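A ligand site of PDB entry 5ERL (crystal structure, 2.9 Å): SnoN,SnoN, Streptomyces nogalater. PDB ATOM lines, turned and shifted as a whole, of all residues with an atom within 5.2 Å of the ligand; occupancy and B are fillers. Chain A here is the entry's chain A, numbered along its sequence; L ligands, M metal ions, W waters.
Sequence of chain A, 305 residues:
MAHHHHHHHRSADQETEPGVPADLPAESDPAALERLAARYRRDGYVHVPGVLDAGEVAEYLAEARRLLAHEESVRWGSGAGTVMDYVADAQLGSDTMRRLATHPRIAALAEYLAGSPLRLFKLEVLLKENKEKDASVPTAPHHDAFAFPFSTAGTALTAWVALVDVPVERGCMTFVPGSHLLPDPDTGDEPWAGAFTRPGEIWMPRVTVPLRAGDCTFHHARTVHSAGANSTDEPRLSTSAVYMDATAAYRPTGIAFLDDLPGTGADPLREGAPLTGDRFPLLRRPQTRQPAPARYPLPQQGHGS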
ATOM      1  N   TRP A  76       0.201   7.435  22.112  1.00  0.00           N
ATOM      2  CA  TRP A  76      -0.003   8.838  22.004  1.00  0.00           C
ATOM      3  C   TRP A  76      -1.079   9.081  23.004  1.00  0.00           C
ATOM      4  O   TRP A  76      -2.155   8.593  22.880  1.00  0.00           O
ATOM      5  CB  TRP A  76      -0.418   9.260  20.617  1.00  0.00           C
ATOM      6  CG  TRP A  76      -0.993  10.698  20.466  1.00  0.00           C
ATOM      7  CD1 TRP A  76      -0.972  11.696  21.428  1.00  0.00           C
ATOM      8  CD2 TRP A  76      -1.548  11.313  19.277  1.00  0.00           C
ATOM      9  NE1 TRP A  76      -1.545  12.854  20.911  1.00  0.00           N
ATOM     10  CE2 TRP A  76      -1.899  12.632  19.618  1.00  0.00           C
ATOM     11  CE3 TRP A  76      -1.791  10.859  17.985  1.00  0.00           C
ATOM     12  CZ2 TRP A  76      -2.431  13.504  18.734  1.00  0.00           C
ATOM     13  CZ3 TRP A  76      -2.372  11.742  17.094  1.00  0.00           C
ATOM     14  CH2 TRP A  76      -2.673  13.050  17.478  1.00  0.00           C
ATOM     15  N   GLY A  77      -0.756   9.810  24.071  1.00  0.00           N
ATOM     16  CA  GLY A  77      -1.592   9.747  25.268  1.00  0.00           C
ATOM     17  C   GLY A  77      -1.352  10.778  26.332  1.00  0.00           C
ATOM     18  O   GLY A  77      -0.397  11.547  26.248  1.00  0.00           O
ATOM     19  N   SER A  78      -2.240  10.834  27.318  1.00  0.00           N
ATOM     20  CA  SER A  78      -2.167  11.822  28.394  1.00  0.00           C
ATOM     21  C   SER A  78      -2.824  11.340  29.643  1.00  0.00           C
ATOM     22  O   SER A  78      -3.460  10.341  29.598  1.00  0.00           O
ATOM     23  CB  SER A  78      -3.019  12.989  27.929  1.00  0.00           C
ATOM     24  OG  SER A  78      -4.234  12.859  28.627  1.00  0.00           O
ATOM     25  N   MET A  84      -4.539   7.404  21.092  1.00  0.00           N
ATOM     26  CA  MET A  84      -4.424   6.176  20.252  1.00  0.00           C
ATOM     27  C   MET A  84      -3.128   5.434  20.546  1.00  0.00           C
ATOM     28  O   MET A  84      -2.199   5.989  21.142  1.00  0.00           O
ATOM     29  CB  MET A  84      -4.454   6.479  18.773  1.00  0.00           C
ATOM     30  CG  MET A  84      -3.267   7.328  18.361  1.00  0.00           C
ATOM     31  SD  MET A  84      -3.263   7.730  16.603  1.00  0.00           S
ATOM     32  CE  MET A  84      -4.632   8.893  16.418  1.00  0.00           C
ATOM     33  N   TYR A  86      -0.367   3.361  18.249  1.00  0.00           N
ATOM     34  CA  TYR A  86      -0.012   3.185  16.866  1.00  0.00           C
ATOM     35  C   TYR A  86       1.343   2.567  16.649  1.00  0.00           C
ATOM     36  O   TYR A  86       2.183   2.517  17.522  1.00  0.00           O
ATOM     37  CB  TYR A  86      -0.028   4.426  16.086  1.00  0.00           C
ATOM     38  CG  TYR A  86       1.046   5.431  16.523  1.00  0.00           C
ATOM     39  CD1 TYR A  86       0.798   6.367  17.551  1.00  0.00           C
ATOM     40  CD2 TYR A  86       2.259   5.545  15.850  1.00  0.00           C
ATOM     41  CE1 TYR A  86       1.727   7.288  17.893  1.00  0.00           C
ATOM     42  CE2 TYR A  86       3.184   6.522  16.180  1.00  0.00           C
ATOM     43  CZ  TYR A  86       2.926   7.379  17.204  1.00  0.00           C
ATOM     44  OH  TYR A  86       3.875   8.285  17.620  1.00  0.00           O
ATOM     45  N   LYS A 122       5.911   8.256   5.539  1.00  0.00           N
ATOM     46  CA  LYS A 122       5.621   7.237   6.551  1.00  0.00           C
ATOM     47  C   LYS A 122       4.218   6.646   6.441  1.00  0.00           C
ATOM     48  O   LYS A 122       3.331   7.264   5.852  1.00  0.00           O
ATOM     49  CB  LYS A 122       5.840   7.795   7.930  1.00  0.00           C
ATOM     50  CG  LYS A 122       4.739   8.645   8.508  1.00  0.00           C
ATOM     51  CD  LYS A 122       5.124   9.073   9.920  1.00  0.00           C
ATOM     52  CE  LYS A 122       4.272  10.316  10.367  1.00  0.00           C
ATOM     53  NZ  LYS A 122       4.261  10.634  11.821  1.00  0.00           N
ATOM     54  N   GLU A 124       1.503   4.551   9.152  1.00  0.00           N
ATOM     55  CA  GLU A 124       1.284   4.217  10.552  1.00  0.00           C
ATOM     56  C   GLU A 124       0.046   3.419  10.710  1.00  0.00           C
ATOM     57  O   GLU A 124      -0.977   3.709  10.086  1.00  0.00           O
ATOM     58  CB  GLU A 124       1.200   5.512  11.447  1.00  0.00           C
ATOM     59  CG  GLU A 124       2.463   6.300  11.450  1.00  0.00           C
ATOM     60  CD  GLU A 124       2.404   7.566  12.292  1.00  0.00           C
ATOM     61  OE1 GLU A 124       1.410   8.342  12.153  1.00  0.00           O
ATOM     62  OE2 GLU A 124       3.403   7.750  13.096  1.00  0.00           O
ATOM     63  N   LEU A 126      -3.007   2.565  12.981  1.00  0.00           N
ATOM     64  CA  LEU A 126      -3.703   3.284  14.099  1.00  0.00           C
ATOM     65  C   LEU A 126      -4.813   2.544  14.867  1.00  0.00           C
ATOM     66  O   LEU A 126      -5.655   1.893  14.250  1.00  0.00           O
ATOM     67  CB  LEU A 126      -4.326   4.595  13.617  1.00  0.00           C
ATOM     68  CG  LEU A 126      -3.471   5.555  12.808  1.00  0.00           C
ATOM     69  CD1 LEU A 126      -4.300   6.827  12.623  1.00  0.00           C
ATOM     70  CD2 LEU A 126      -2.126   5.884  13.436  1.00  0.00           C
ATOM     71  N   ALA A 140      -7.515  15.542  19.594  1.00  0.00           N
ATOM     72  CA  ALA A 140      -7.874  16.947  19.669  1.00  0.00           C
ATOM     73  C   ALA A 140      -7.576  17.639  18.345  1.00  0.00           C
ATOM     74  O   ALA A 140      -6.800  17.133  17.567  1.00  0.00           O
ATOM     75  CB  ALA A 140      -7.166  17.598  20.824  1.00  0.00           C
ATOM     76  N   HIS A 142      -5.968  19.707  15.527  1.00  0.00           N
ATOM     77  CA  HIS A 142      -4.574  19.927  15.320  1.00  0.00           C
ATOM     78  C   HIS A 142      -4.309  20.167  13.851  1.00  0.00           C
ATOM     79  O   HIS A 142      -5.178  20.284  13.066  1.00  0.00           O
ATOM     80  CB  HIS A 142      -3.771  18.749  15.870  1.00  0.00           C
ATOM     81  CG  HIS A 142      -3.879  17.501  15.078  1.00  0.00           C
ATOM     82  ND1 HIS A 142      -4.946  16.650  15.129  1.00  0.00           N
ATOM     83  CD2 HIS A 142      -3.064  17.025  14.132  1.00  0.00           C
ATOM     84  CE1 HIS A 142      -4.740  15.659  14.289  1.00  0.00           C
ATOM     85  NE2 HIS A 142      -3.677  15.943  13.573  1.00  0.00           N
ATOM     86  N   ASP A 144      -1.379  19.227  11.272  1.00  0.00           N
ATOM     87  CA  ASP A 144      -0.238  18.272  11.092  1.00  0.00           C
ATOM     88  C   ASP A 144       1.034  18.833  10.455  1.00  0.00           C
ATOM     89  O   ASP A 144       2.149  18.418  10.709  1.00  0.00           O
ATOM     90  CB  ASP A 144      -0.689  17.032  10.276  1.00  0.00           C
ATOM     91  CG  ASP A 144      -1.440  16.003  11.130  1.00  0.00           C
ATOM     92  OD1 ASP A 144      -0.917  15.641  12.192  1.00  0.00           O
ATOM     93  OD2 ASP A 144      -2.472  15.492  10.639  1.00  0.00           O
ATOM     94  N   ALA A 147       4.817  19.632  11.829  1.00  0.00           N
ATOM     95  CA  ALA A 147       5.231  18.439  12.588  1.00  0.00           C
ATOM     96  C   ALA A 147       5.825  17.333  11.707  1.00  0.00           C
ATOM     97  O   ALA A 147       6.168  16.285  12.163  1.00  0.00           O
ATOM     98  CB  ALA A 147       4.063  17.876  13.336  1.00  0.00           C
ATOM     99  N   PHE A 148       5.909  17.609  10.430  1.00  0.00           N
ATOM    100  CA  PHE A 148       6.567  16.705   9.478  1.00  0.00           C
ATOM    101  C   PHE A 148       7.970  17.224   9.270  1.00  0.00           C
ATOM    102  O   PHE A 148       8.123  18.355   8.866  1.00  0.00           O
ATOM    103  CB  PHE A 148       5.845  16.698   8.125  1.00  0.00           C
ATOM    104  CG  PHE A 148       4.456  16.093   8.184  1.00  0.00           C
ATOM    105  CD1 PHE A 148       4.176  14.997   8.900  1.00  0.00           C
ATOM    106  CD2 PHE A 148       3.422  16.693   7.507  1.00  0.00           C
ATOM    107  CE1 PHE A 148       2.896  14.521   8.975  1.00  0.00           C
ATOM    108  CE2 PHE A 148       2.146  16.179   7.546  1.00  0.00           C
ATOM    109  CZ  PHE A 148       1.890  15.109   8.291  1.00  0.00           C
ATOM    110  N   GLU A 190       5.154  23.872  19.630  1.00  0.00           N
ATOM    111  CA  GLU A 190       4.705  22.510  19.341  1.00  0.00           C
ATOM    112  C   GLU A 190       4.178  22.540  17.938  1.00  0.00           C
ATOM    113  O   GLU A 190       3.147  23.132  17.705  1.00  0.00           O
ATOM    114  CB  GLU A 190       3.632  21.939  20.266  1.00  0.00           C
ATOM    115  CG  GLU A 190       4.253  21.348  21.532  1.00  0.00           C
ATOM    116  CD  GLU A 190       3.918  22.191  22.710  1.00  0.00           C
ATOM    117  OE1 GLU A 190       2.826  22.794  22.717  1.00  0.00           O
ATOM    118  OE2 GLU A 190       4.758  22.297  23.599  1.00  0.00           O
ATOM    119  N   TRP A 192       2.551  20.982  15.800  1.00  0.00           N
ATOM    120  CA  TRP A 192       1.121  20.606  15.528  1.00  0.00           C
ATOM    121  C   TRP A 192       0.069  21.606  16.084  1.00  0.00           C
ATOM    122  O   TRP A 192      -1.117  21.494  15.754  1.00  0.00           O
ATOM    123  CB  TRP A 192       0.799  19.222  16.107  1.00  0.00           C
ATOM    124  CG  TRP A 192       1.107  19.118  17.583  1.00  0.00           C
ATOM    125  CD1 TRP A 192       0.431  19.710  18.597  1.00  0.00           C
ATOM    126  CD2 TRP A 192       2.184  18.401  18.189  1.00  0.00           C
ATOM    127  NE1 TRP A 192       1.016  19.407  19.796  1.00  0.00           N
ATOM    128  CE2 TRP A 192       2.093  18.593  19.560  1.00  0.00           C
ATOM    129  CE3 TRP A 192       3.223  17.597  17.686  1.00  0.00           C
ATOM    130  CZ2 TRP A 192       2.980  18.045  20.453  1.00  0.00           C
ATOM    131  CZ3 TRP A 192       4.087  17.034  18.568  1.00  0.00           C
ATOM    132  CH2 TRP A 192       3.970  17.257  19.934  1.00  0.00           C
ATOM    133  N   SER A 240      -2.689   5.409   8.389  1.00  0.00           N
ATOM    134  CA  SER A 240      -2.438   6.816   7.998  1.00  0.00           C
ATOM    135  C   SER A 240      -1.106   6.910   7.330  1.00  0.00           C
ATOM    136  O   SER A 240      -0.116   6.615   7.913  1.00  0.00           O
ATOM    137  CB  SER A 240      -2.428   7.738   9.231  1.00  0.00           C
ATOM    138  OG  SER A 240      -2.515   9.103   8.856  1.00  0.00           O
ATOM    139  N   VAL A 242       1.534   9.352   5.236  1.00  0.00           N
ATOM    140  CA  VAL A 242       1.904  10.665   4.851  1.00  0.00           C
ATOM    141  C   VAL A 242       2.691  10.612   3.566  1.00  0.00           C
ATOM    142  O   VAL A 242       3.821  10.147   3.541  1.00  0.00           O
ATOM    143  CB  VAL A 242       2.706  11.346   5.994  1.00  0.00           C
ATOM    144  CG1 VAL A 242       3.210  12.746   5.647  1.00  0.00           C
ATOM    145  CG2 VAL A 242       1.846  11.472   7.238  1.00  0.00           C
ATOM    146  N   PHE A 257      11.339  13.002  19.101  1.00  0.00           N
ATOM    147  CA  PHE A 257      10.630  11.847  18.681  1.00  0.00           C
ATOM    148  C   PHE A 257      10.018  12.002  17.270  1.00  0.00           C
ATOM    149  O   PHE A 257       9.749  10.960  16.588  1.00  0.00           O
ATOM    150  CB  PHE A 257       9.603  11.370  19.691  1.00  0.00           C
ATOM    151  CG  PHE A 257       8.289  12.070  19.618  1.00  0.00           C
ATOM    152  CD1 PHE A 257       7.347  11.748  18.660  1.00  0.00           C
ATOM    153  CD2 PHE A 257       7.960  13.025  20.560  1.00  0.00           C
ATOM    154  CE1 PHE A 257       6.109  12.402  18.621  1.00  0.00           C
ATOM    155  CE2 PHE A 257       6.741  13.666  20.538  1.00  0.00           C
ATOM    156  CZ  PHE A 257       5.802  13.363  19.567  1.00  0.00           C
ATOM    157  N   LEU A 258       9.842  13.247  16.804  1.00  0.00           N
ATOM    158  CA  LEU A 258       9.435  13.512  15.378  1.00  0.00           C
ATOM    159  C   LEU A 258      10.588  13.483  14.363  1.00  0.00           C
ATOM    160  O   LEU A 258      10.445  13.059  13.225  1.00  0.00           O
ATOM    161  CB  LEU A 258       8.756  14.842  15.236  1.00  0.00           C
ATOM    162  CG  LEU A 258       7.449  14.996  15.980  1.00  0.00           C
ATOM    163  CD1 LEU A 258       6.905  16.413  15.912  1.00  0.00           C
ATOM    164  CD2 LEU A 258       6.433  14.005  15.412  1.00  0.00           C
HETATM  165  C1  LIG L   1      -2.332  19.002  23.849  1.00  0.00           C
HETATM  166  C2  LIG L   1      -3.144  19.442  25.022  1.00  0.00           C
HETATM  167  O1  LIG L   1      -2.257  19.438  26.222  1.00  0.00           O
HETATM  168  C3  LIG L   1      -4.482  18.397  24.972  1.00  0.00           C
HETATM  169  O2  LIG L   1      -5.257  18.514  23.659  1.00  0.00           O
HETATM  170  C4  LIG L   1      -4.141  16.840  25.250  1.00  0.00           C
HETATM  171  C5  LIG L   1      -3.656  16.617  26.742  1.00  0.00           C
HETATM  172  O3  LIG L   1      -3.183  16.405  24.206  1.00  0.00           O
HETATM  173  C6  LIG L   1      -1.983  17.506  24.106  1.00  0.00           C
HETATM  174  O4  LIG L   1      -1.085  17.225  23.097  1.00  0.00           O
HETATM  175  C7  LIG L   1      -0.002  16.381  23.470  1.00  0.00           C
HETATM  176  C8  LIG L   1      -0.110  15.385  24.718  1.00  0.00           C
HETATM  177  C9  LIG L   1       1.313  14.931  24.999  1.00  0.00           C
HETATM  178  C10 LIG L   1       1.525  14.063  26.272  1.00  0.00           C
HETATM  179  O5  LIG L   1       1.890  16.124  25.223  1.00  0.00           O
HETATM  180  C11 LIG L   1       0.425  15.687  22.320  1.00  0.00           C
HETATM  181  C12 LIG L   1      -0.027  15.966  20.995  1.00  0.00           C
HETATM  182  O6  LIG L   1      -0.934  16.894  20.731  1.00  0.00           O
HETATM  183  C13 LIG L   1       0.453  15.372  19.863  1.00  0.00           C
HETATM  184  C14 LIG L   1      -0.032  15.761  18.618  1.00  0.00           C
HETATM  185  O7  LIG L   1      -0.901  16.624  18.539  1.00  0.00           O
HETATM  186  C15 LIG L   1       0.504  15.056  17.477  1.00  0.00           C
HETATM  187  C16 LIG L   1       0.110  15.382  16.197  1.00  0.00           C
HETATM  188  O8  LIG L   1      -0.816  16.358  16.069  1.00  0.00           O
HETATM  189  C17 LIG L   1       0.623  14.715  15.115  1.00  0.00           C
HETATM  190  C18 LIG L   1       1.597  13.719  15.209  1.00  0.00           C
HETATM  191  C19 LIG L   1       2.198  12.990  13.998  1.00  0.00           C
HETATM  192  C20 LIG L   1       2.680  14.088  12.986  1.00  0.00           C
HETATM  193  O9  LIG L   1       3.344  12.222  14.161  1.00  0.00           O
HETATM  194  C21 LIG L   1       1.301  12.056  13.424  1.00  0.00           C
HETATM  195  O10 LIG L   1       1.712  11.679  12.118  1.00  0.00           O
HETATM  196  C22 LIG L   1       1.135  10.980  14.477  1.00  0.00           C
HETATM  197  N1  LIG L   1       0.391   9.800  14.028  1.00  0.00           N
HETATM  198  C23 LIG L   1       0.242   8.769  15.099  1.00  0.00           C
HETATM  199  C24 LIG L   1      -0.904  10.086  13.400  1.00  0.00           C
HETATM  200  C25 LIG L   1       2.474  10.622  15.169  1.00  0.00           C
HETATM  201  C26 LIG L   1       3.363  11.668  15.362  1.00  0.00           C
HETATM  202  O11 LIG L   1       2.939  12.439  16.597  1.00  0.00           O
HETATM  203  C27 LIG L   1       1.995  13.428  16.489  1.00  0.00           C
HETATM  204  C28 LIG L   1       1.487  14.046  17.610  1.00  0.00           C
HETATM  205  C29 LIG L   1       1.945  13.674  18.889  1.00  0.00           C
HETATM  206  O12 LIG L   1       2.785  12.800  19.030  1.00  0.00           O
HETATM  207  C30 LIG L   1       1.418  14.370  20.024  1.00  0.00           C
HETATM  208  C31 LIG L   1       1.868  14.077  21.351  1.00  0.00           C
HETATM  209  C32 LIG L   1       1.424  14.707  22.531  1.00  0.00           C
HETATM  210  C33 LIG L   1       2.011  14.319  23.806  1.00  0.00           C
HETATM  211  C34 LIG L   1       3.391  14.810  23.946  1.00  0.00           C
HETATM  212  O13 LIG L   1       4.281  14.329  24.657  1.00  0.00           O
HETATM  213  O14 LIG L   1       3.576  16.137  23.396  1.00  0.00           O
HETATM  214  C35 LIG L   1       4.983  16.577  23.328  1.00  0.00           C
HETATM  215 NI    NI M   1      -3.593  14.735  12.035  1.00  0.00          NI
HETATM  216  O   HOH W   1       0.254   9.758   9.759  1.00  0.00           O
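OE2 of Glu 124 is in salt-bridge range of NZ of Lys 122, at 3.3 Å. The backbone NH (N) of Glu 124 lies within hydrogen-bond range of the backbone carbonyl oxygen (O) of Ser 240 (2.9 Å). The backbone carbonyl oxygen (O) of Lys 122 sits at hydrogen-bond distance from the backbone NH (N) of Val 242. The backbone carbonyl oxygen (O) of Ala 140 is in hydrogen-bond range of a ring nitrogen (ND1) of His 142, at 3.1 Å. N of Trp 76 sits at hydrogen-bond distance from O of Met 84 (3.0 Å).
The side-chain carboxylate of Glu 124 is in salt-bridge range of a nitrogen (N1) of the ligand (2.6 Å). O10 of the ligand sits at hydrogen-bond distance from NZ of Lys 122 (2.8 Å). An oxygen (O6) of the ligand lies within hydrogen-bond range of the indole nitrogen (NE1) of Trp 192 (3.3 Å).
Water W1 lies within hydrogen-bond range of the side-chain hydroxyl of Ser 240, the side-chain carboxylate of Glu 124 and an oxygen (O10) of the ligand.
CZ2 of Trp 76 touches C14 of the ligand, 3.3 Å away. Gly 77 touches the ligand (O to C10, 3.2 Å). Ser 78 touches the ligand (CB to C5, 3.9 Å). Met 84 touches the ligand. Tyr 86 touches the ligand. Ala 140 touches the ligand. His 142 touches the ligand. OD1 of Asp 144 touches C17 of the ligand, 3.4 Å away. Phe 257 touches the ligand (CZ to O12, 3.1 Å). Leu 258 touches the ligand (CD2 to O9, 3.8 Å). Within 4 Å of the ligand: Trp 76, Gly 77, Ser 78, Met 84, Tyr 86, Lys 122, Glu 124, Ala 140, His 142, Asp 144, Trp 192, Phe 257 and Leu 258. The nearest printed residue that does not touch the ligand is Phe 148 (4.04 Å).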
